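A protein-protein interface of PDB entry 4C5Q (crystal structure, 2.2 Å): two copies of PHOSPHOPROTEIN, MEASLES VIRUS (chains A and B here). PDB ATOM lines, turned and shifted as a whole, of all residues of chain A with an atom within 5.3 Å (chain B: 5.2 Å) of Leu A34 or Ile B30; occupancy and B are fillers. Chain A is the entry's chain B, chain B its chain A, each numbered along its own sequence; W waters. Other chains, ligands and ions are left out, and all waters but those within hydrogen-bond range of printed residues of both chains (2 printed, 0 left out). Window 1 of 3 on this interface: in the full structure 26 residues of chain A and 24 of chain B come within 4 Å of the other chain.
Asn A27 touches Asn B27 (ND2 to OD1, 3.98 Å). Ile B30 touches Ile A30 (CD1 to CG2, 3.5 Å). Ile A31 touches Asp B26. Leu A34 touches Ile B30. Leu A34 touches Lys B33 (CB to CD, 3.6 Å). Leu B34 touches Leu A34. Leu A34 touches Leu B37. Leu A37 touches Leu B37. Lys B33 touches Leu A38. Leu B37 touches Leu A38.
The side-chain amino group (NZ) of Lys B33 lies within salt-bridge range of the side-chain carboxylate (OE1) of Glu A35.
Ile A31 touches Ile B30, but with the chains exchanged Ile A30 does not touch Ile B31 (7.8 Å). Leu A34 touches Ile B30, but with the chains exchanged Ile A30 does not touch Leu B34 (6.8 Å). Leu A34 touches Lys B33, but with the chains exchanged Lys A33 does not touch Leu B34 (8.5 Å). Leu A34 touches its own counterpart, Leu B34. Positions printed for both chains: 27, 29, 30, 31, 32, 33, 34, 35 and 37. Of the 12 pairs that touch across the chains among the printed residues, 4 have their exchanged pair printed and touching as well.
Of the printed residues of chain B, Asn A27 touches Asn B27 (3.98 Å). Of the printed residues of chain B, Ile A30 touches Ile B30 (3.5 Å). Leu A34 touches just these residues of chain B: Ile B30 (3.5 Å), Lys B33 (3.6 Å), Leu B34 (3.6 Å) and Leu B37 (3.6 Å). Printed residues of chain B within 4 Å of Leu A37: Leu B37. Ile B30 touches just these residues of chain A: Ile A30, Ile A31 and Leu A34.
Of the 11 printed residues of chain A, 7 touch a printed residue of chain B. Printed residues of chain A that touch a printed residue of chain B: Asn A27, Ile A30, Ile A31, Leu A34, Glu A35, Leu A37 and Leu A38. Hydrophobic or aromatic side chains of chain A within 4 Å of the printed part of chain B: Ile A30, Ile A31, Leu A34, Leu A37 and Leu A38. Hydrophobic or aromatic side chains of chain B that line the printed part of chain A: Ile B30, Leu B34 and Leu B37. Among the printed residues, 12 pairs touch across the chains. Among the printed residues, Asp or Glu carboxylates within 4 Å of a Lys or Arg side-chain nitrogen of the other chain: Glu A35 with Lys B33.
Water W2 bridges OD2 of Asp B26 and ND2 of Asn A27. Water W1 bridges OD1 of Asn B27 (3.2 Å) and OD1 of Asn A27 (3.3 Å).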
ATOM      1  N   ASN A  27      24.010  12.406  14.397  1.00  0.00           N
ATOM      2  CA  ASN A  27      23.161  11.519  13.595  1.00  0.00           C
ATOM      3  C   ASN A  27      21.661  11.825  13.659  1.00  0.00           C
ATOM      4  O   ASN A  27      20.986  11.783  12.639  1.00  0.00           O
ATOM      5  CB  ASN A  27      23.450  10.058  13.891  1.00  0.00           C
ATOM      6  CG  ASN A  27      24.734   9.591  13.242  1.00  0.00           C
ATOM      7  OD1 ASN A  27      25.243  10.244  12.335  1.00  0.00           O
ATOM      8  ND2 ASN A  27      25.272   8.470  13.712  1.00  0.00           N
ATOM      9  N   LYS A  29      20.279  14.779  14.296  1.00  0.00           N
ATOM     10  CA  LYS A  29      20.131  16.019  13.559  1.00  0.00           C
ATOM     11  C   LYS A  29      20.262  15.794  12.043  1.00  0.00           C
ATOM     12  O   LYS A  29      19.501  16.358  11.235  1.00  0.00           O
ATOM     13  CB  LYS A  29      21.173  17.029  14.061  1.00  0.00           C
ATOM     14  CG  LYS A  29      21.453  18.155  13.094  1.00  0.00           C
ATOM     15  CD  LYS A  29      22.722  18.921  13.452  1.00  0.00           C
ATOM     16  CE  LYS A  29      22.619  19.550  14.821  1.00  0.00           C
ATOM     17  NZ  LYS A  29      21.538  20.573  14.895  1.00  0.00           N
ATOM     18  N   ILE A  30      21.223  14.965  11.651  1.00  0.00           N
ATOM     19  CA  ILE A  30      21.345  14.591  10.248  1.00  0.00           C
ATOM     20  C   ILE A  30      20.046  13.916   9.750  1.00  0.00           C
ATOM     21  O   ILE A  30      19.547  14.228   8.661  1.00  0.00           O
ATOM     22  CB  ILE A  30      22.578  13.674  10.021  1.00  0.00           C
ATOM     23  CG1 ILE A  30      23.874  14.471  10.124  1.00  0.00           C
ATOM     24  CG2 ILE A  30      22.530  13.001   8.666  1.00  0.00           C
ATOM     25  CD1 ILE A  30      25.134  13.587  10.258  1.00  0.00           C
ATOM     26  N   ILE A  31      19.483  13.018  10.552  1.00  0.00           N
ATOM     27  CA  ILE A  31      18.285  12.277  10.114  1.00  0.00           C
ATOM     28  C   ILE A  31      17.099  13.191   9.841  1.00  0.00           C
ATOM     29  O   ILE A  31      16.373  12.993   8.864  1.00  0.00           O
ATOM     30  CB  ILE A  31      17.874  11.193  11.131  1.00  0.00           C
ATOM     31  CG1 ILE A  31      18.858  10.026  11.080  1.00  0.00           C
ATOM     32  CG2 ILE A  31      16.465  10.673  10.850  1.00  0.00           C
ATOM     33  CD1 ILE A  31      18.747   9.073  12.248  1.00  0.00           C
ATOM     34  N   SER A  32      16.899  14.184  10.708  1.00  0.00           N
ATOM     35  CA  SER A  32      15.745  15.069  10.584  1.00  0.00           C
ATOM     36  C   SER A  32      15.912  16.044   9.425  1.00  0.00           C
ATOM     37  O   SER A  32      14.933  16.354   8.738  1.00  0.00           O
ATOM     38  CB  SER A  32      15.464  15.812  11.897  1.00  0.00           C
ATOM     39  OG  SER A  32      16.590  16.541  12.351  1.00  0.00           O
ATOM     40  N   LYS A  33      17.141  16.523   9.213  1.00  0.00           N
ATOM     41  CA  LYS A  33      17.456  17.319   8.027  1.00  0.00           C
ATOM     42  C   LYS A  33      17.120  16.531   6.761  1.00  0.00           C
ATOM     43  O   LYS A  33      16.497  17.070   5.833  1.00  0.00           O
ATOM     44  CB  LYS A  33      18.928  17.734   8.009  1.00  0.00           C
ATOM     45  CG  LYS A  33      19.295  18.757   9.066  1.00  0.00           C
ATOM     46  CD  LYS A  33      20.664  19.370   8.778  1.00  0.00           C
ATOM     47  CE  LYS A  33      21.007  20.446   9.806  1.00  0.00           C
ATOM     48  NZ  LYS A  33      20.118  21.645   9.679  1.00  0.00           N
ATOM     49  N   LEU A  34      17.533  15.263   6.724  1.00  0.00           N
ATOM     50  CA  LEU A  34      17.208  14.386   5.594  1.00  0.00           C
ATOM     51  C   LEU A  34      15.708  14.170   5.405  1.00  0.00           C
ATOM     52  O   LEU A  34      15.231  14.161   4.270  1.00  0.00           O
ATOM     53  CB  LEU A  34      17.929  13.045   5.700  1.00  0.00           C
ATOM     54  CG  LEU A  34      19.429  13.125   5.415  1.00  0.00           C
ATOM     55  CD1 LEU A  34      20.120  11.833   5.773  1.00  0.00           C
ATOM     56  CD2 LEU A  34      19.661  13.450   3.962  1.00  0.00           C
ATOM     57  N   GLU A  35      14.965  14.019   6.503  1.00  0.00           N
ATOM     58  CA  GLU A  35      13.505  13.881   6.423  1.00  0.00           C
ATOM     59  C   GLU A  35      12.874  15.142   5.863  1.00  0.00           C
ATOM     60  O   GLU A  35      11.837  15.093   5.197  1.00  0.00           O
ATOM     61  CB  GLU A  35      12.913  13.624   7.807  1.00  0.00           C
ATOM     62  CG  GLU A  35      13.210  12.242   8.378  1.00  0.00           C
ATOM     63  CD  GLU A  35      12.268  11.158   7.855  1.00  0.00           C
ATOM     64  OE1 GLU A  35      11.848  11.203   6.668  1.00  0.00           O
ATOM     65  OE2 GLU A  35      11.967  10.236   8.640  1.00  0.00           O
ATOM     66  N   SER A  36      13.506  16.275   6.148  1.00  0.00           N
ATOM     67  CA  SER A  36      13.032  17.547   5.668  1.00  0.00           C
ATOM     68  C   SER A  36      13.349  17.701   4.187  1.00  0.00           C
ATOM     69  O   SER A  36      12.563  18.262   3.441  1.00  0.00           O
ATOM     70  CB  SER A  36      13.682  18.676   6.462  1.00  0.00           C
ATOM     71  OG  SER A  36      13.383  19.924   5.868  1.00  0.00           O
ATOM     72  N   LEU A  37      14.506  17.204   3.761  1.00  0.00           N
ATOM     73  CA  LEU A  37      14.883  17.275   2.354  1.00  0.00           C
ATOM     74  C   LEU A  37      14.035  16.330   1.495  1.00  0.00           C
ATOM     75  O   LEU A  37      13.760  16.624   0.329  1.00  0.00           O
ATOM     76  CB  LEU A  37      16.378  16.958   2.167  1.00  0.00           C
ATOM     77  CG  LEU A  37      17.412  18.039   2.477  1.00  0.00           C
ATOM     78  CD1 LEU A  37      18.821  17.442   2.516  1.00  0.00           C
ATOM     79  CD2 LEU A  37      17.327  19.168   1.458  1.00  0.00           C
ATOM     80  N   LEU A  38      13.625  15.199   2.063  1.00  0.00           N
ATOM     81  CA  LEU A  38      12.807  14.231   1.319  1.00  0.00           C
ATOM     82  C   LEU A  38      11.468  14.806   0.839  1.00  0.00           C
ATOM     83  O   LEU A  38      10.910  14.326  -0.143  1.00  0.00           O
ATOM     84  CB  LEU A  38      12.572  12.985   2.148  1.00  0.00           C
ATOM     85  CG  LEU A  38      13.779  12.062   2.309  1.00  0.00           C
ATOM     86  CD1 LEU A  38      13.463  11.025   3.360  1.00  0.00           C
ATOM     87  CD2 LEU A  38      14.125  11.384   0.989  1.00  0.00           C
ATOM     88  N   ASP B  26      21.588   3.807  12.195  1.00  0.00           N
ATOM     89  CA  ASP B  26      21.274   5.158  11.772  1.00  0.00           C
ATOM     90  C   ASP B  26      21.976   5.475  10.456  1.00  0.00           C
ATOM     91  O   ASP B  26      21.404   6.110   9.575  1.00  0.00           O
ATOM     92  CB  ASP B  26      21.687   6.144  12.856  1.00  0.00           C
ATOM     93  CG  ASP B  26      20.597   6.361  13.876  1.00  0.00           C
ATOM     94  OD1 ASP B  26      19.558   5.681  13.775  1.00  0.00           O
ATOM     95  OD2 ASP B  26      20.773   7.210  14.772  1.00  0.00           O
ATOM     96  N   ASN B  27      23.209   5.012  10.311  1.00  0.00           N
ATOM     97  CA  ASN B  27      23.893   5.187   9.042  1.00  0.00           C
ATOM     98  C   ASN B  27      23.191   4.481   7.886  1.00  0.00           C
ATOM     99  O   ASN B  27      23.147   4.996   6.775  1.00  0.00           O
ATOM    100  CB  ASN B  27      25.361   4.799   9.150  1.00  0.00           C
ATOM    101  CG  ASN B  27      26.170   5.825   9.926  1.00  0.00           C
ATOM    102  OD1 ASN B  27      25.764   6.982  10.050  1.00  0.00           O
ATOM    103  ND2 ASN B  27      27.320   5.406  10.453  1.00  0.00           N
ATOM    104  N   GLN B  28      22.601   3.327   8.154  1.00  0.00           N
ATOM    105  CA  GLN B  28      21.854   2.629   7.114  1.00  0.00           C
ATOM    106  C   GLN B  28      20.594   3.407   6.749  1.00  0.00           C
ATOM    107  O   GLN B  28      20.251   3.480   5.570  1.00  0.00           O
ATOM    108  CB  GLN B  28      21.520   1.200   7.532  1.00  0.00           C
ATOM    109  CG  GLN B  28      22.739   0.436   8.061  1.00  0.00           C
ATOM    110  CD  GLN B  28      23.976   0.686   7.234  1.00  0.00           C
ATOM    111  OE1 GLN B  28      24.009   0.390   6.041  1.00  0.00           O
ATOM    112  NE2 GLN B  28      25.002   1.250   7.859  1.00  0.00           N
ATOM    113  N   LYS B  29      19.927   4.017   7.737  1.00  0.00           N
ATOM    114  CA  LYS B  29      18.812   4.921   7.422  1.00  0.00           C
ATOM    115  C   LYS B  29      19.269   6.117   6.592  1.00  0.00           C
ATOM    116  O   LYS B  29      18.604   6.487   5.610  1.00  0.00           O
ATOM    117  CB  LYS B  29      18.147   5.481   8.678  1.00  0.00           C
ATOM    118  CG  LYS B  29      17.683   4.482   9.689  1.00  0.00           C
ATOM    119  CD  LYS B  29      17.009   5.218  10.836  1.00  0.00           C
ATOM    120  CE  LYS B  29      15.944   6.181  10.322  1.00  0.00           C
ATOM    121  NZ  LYS B  29      14.809   5.450   9.693  1.00  0.00           N
ATOM    122  N   ILE B  30      20.371   6.748   7.017  1.00  0.00           N
ATOM    123  CA  ILE B  30      20.949   7.877   6.280  1.00  0.00           C
ATOM    124  C   ILE B  30      21.164   7.496   4.808  1.00  0.00           C
ATOM    125  O   ILE B  30      20.684   8.168   3.891  1.00  0.00           O
ATOM    126  CB  ILE B  30      22.317   8.342   6.881  1.00  0.00           C
ATOM    127  CG1 ILE B  30      22.173   8.844   8.308  1.00  0.00           C
ATOM    128  CG2 ILE B  30      22.920   9.454   6.069  1.00  0.00           C
ATOM    129  CD1 ILE B  30      21.102   9.837   8.443  1.00  0.00           C
ATOM    130  N   ILE B  31      21.871   6.395   4.594  1.00  0.00           N
ATOM    131  CA  ILE B  31      22.208   5.963   3.236  1.00  0.00           C
ATOM    132  C   ILE B  31      21.002   5.804   2.315  1.00  0.00           C
ATOM    133  O   ILE B  31      21.039   6.242   1.164  1.00  0.00           O
ATOM    134  CB  ILE B  31      23.013   4.666   3.265  1.00  0.00           C
ATOM    135  CG1 ILE B  31      24.390   4.931   3.872  1.00  0.00           C
ATOM    136  CG2 ILE B  31      23.187   4.099   1.861  1.00  0.00           C
ATOM    137  CD1 ILE B  31      25.070   3.676   4.427  1.00  0.00           C
ATOM    138  N   SER B  32      19.936   5.177   2.815  1.00  0.00           N
ATOM    139  CA  SER B  32      18.768   4.902   1.983  1.00  0.00           C
ATOM    140  C   SER B  32      17.927   6.159   1.737  1.00  0.00           C
ATOM    141  O   SER B  32      17.270   6.281   0.701  1.00  0.00           O
ATOM    142  CB  SER B  32      17.915   3.785   2.586  1.00  0.00           C
ATOM    143  OG  SER B  32      17.409   4.148   3.853  1.00  0.00           O
ATOM    144  N   LYS B  33      17.948   7.091   2.688  1.00  0.00           N
ATOM    145  CA  LYS B  33      17.302   8.384   2.489  1.00  0.00           C
ATOM    146  C   LYS B  33      18.033   9.124   1.372  1.00  0.00           C
ATOM    147  O   LYS B  33      17.413   9.760   0.503  1.00  0.00           O
ATOM    148  CB  LYS B  33      17.344   9.208   3.769  1.00  0.00           C
ATOM    149  CG  LYS B  33      16.367   8.759   4.840  1.00  0.00           C
ATOM    150  CD  LYS B  33      16.359   9.764   6.001  1.00  0.00           C
ATOM    151  CE  LYS B  33      15.284   9.423   7.004  1.00  0.00           C
ATOM    152  NZ  LYS B  33      13.966   9.396   6.314  1.00  0.00           N
ATOM    153  N   LEU B  34      19.356   9.023   1.401  1.00  0.00           N
ATOM    154  CA  LEU B  34      20.203   9.590   0.359  1.00  0.00           C
ATOM    155  C   LEU B  34      19.972   8.952  -1.000  1.00  0.00           C
ATOM    156  O   LEU B  34      19.878   9.665  -2.003  1.00  0.00           O
ATOM    157  CB  LEU B  34      21.674   9.483   0.748  1.00  0.00           C
ATOM    158  CG  LEU B  34      21.937  10.382   1.946  1.00  0.00           C
ATOM    159  CD1 LEU B  34      23.301  10.112   2.540  1.00  0.00           C
ATOM    160  CD2 LEU B  34      21.800  11.813   1.527  1.00  0.00           C
ATOM    161  N   GLU B  35      19.884   7.621  -1.041  1.00  0.00           N
ATOM    162  CA  GLU B  35      19.546   6.937  -2.295  1.00  0.00           C
ATOM    163  C   GLU B  35      18.228   7.477  -2.833  1.00  0.00           C
ATOM    164  O   GLU B  35      18.078   7.705  -4.027  1.00  0.00           O
ATOM    165  CB  GLU B  35      19.444   5.426  -2.100  1.00  0.00           C
ATOM    166  CG  GLU B  35      20.774   4.718  -1.776  1.00  0.00           C
ATOM    167  CD  GLU B  35      21.756   4.642  -2.955  1.00  0.00           C
ATOM    168  OE1 GLU B  35      21.554   5.311  -4.004  1.00  0.00           O
ATOM    169  OE2 GLU B  35      22.757   3.903  -2.819  1.00  0.00           O
ATOM    170  N   LEU B  37      16.922  10.504  -2.146  1.00  0.00           N
ATOM    171  CA  LEU B  37      17.102  11.894  -2.551  1.00  0.00           C
ATOM    172  C   LEU B  37      17.829  12.038  -3.885  1.00  0.00           C
ATOM    173  O   LEU B  37      17.549  12.967  -4.651  1.00  0.00           O
ATOM    174  CB  LEU B  37      17.861  12.681  -1.471  1.00  0.00           C
ATOM    175  CG  LEU B  37      17.024  13.072  -0.262  1.00  0.00           C
ATOM    176  CD1 LEU B  37      17.904  13.565   0.857  1.00  0.00           C
ATOM    177  CD2 LEU B  37      15.996  14.133  -0.667  1.00  0.00           C
HETATM  178  O   HOH W   1      27.988   8.578  11.619  1.00  0.00           O
HETATM  179  O   HOH W   2      23.313   7.058  15.903  1.00  0.00           O
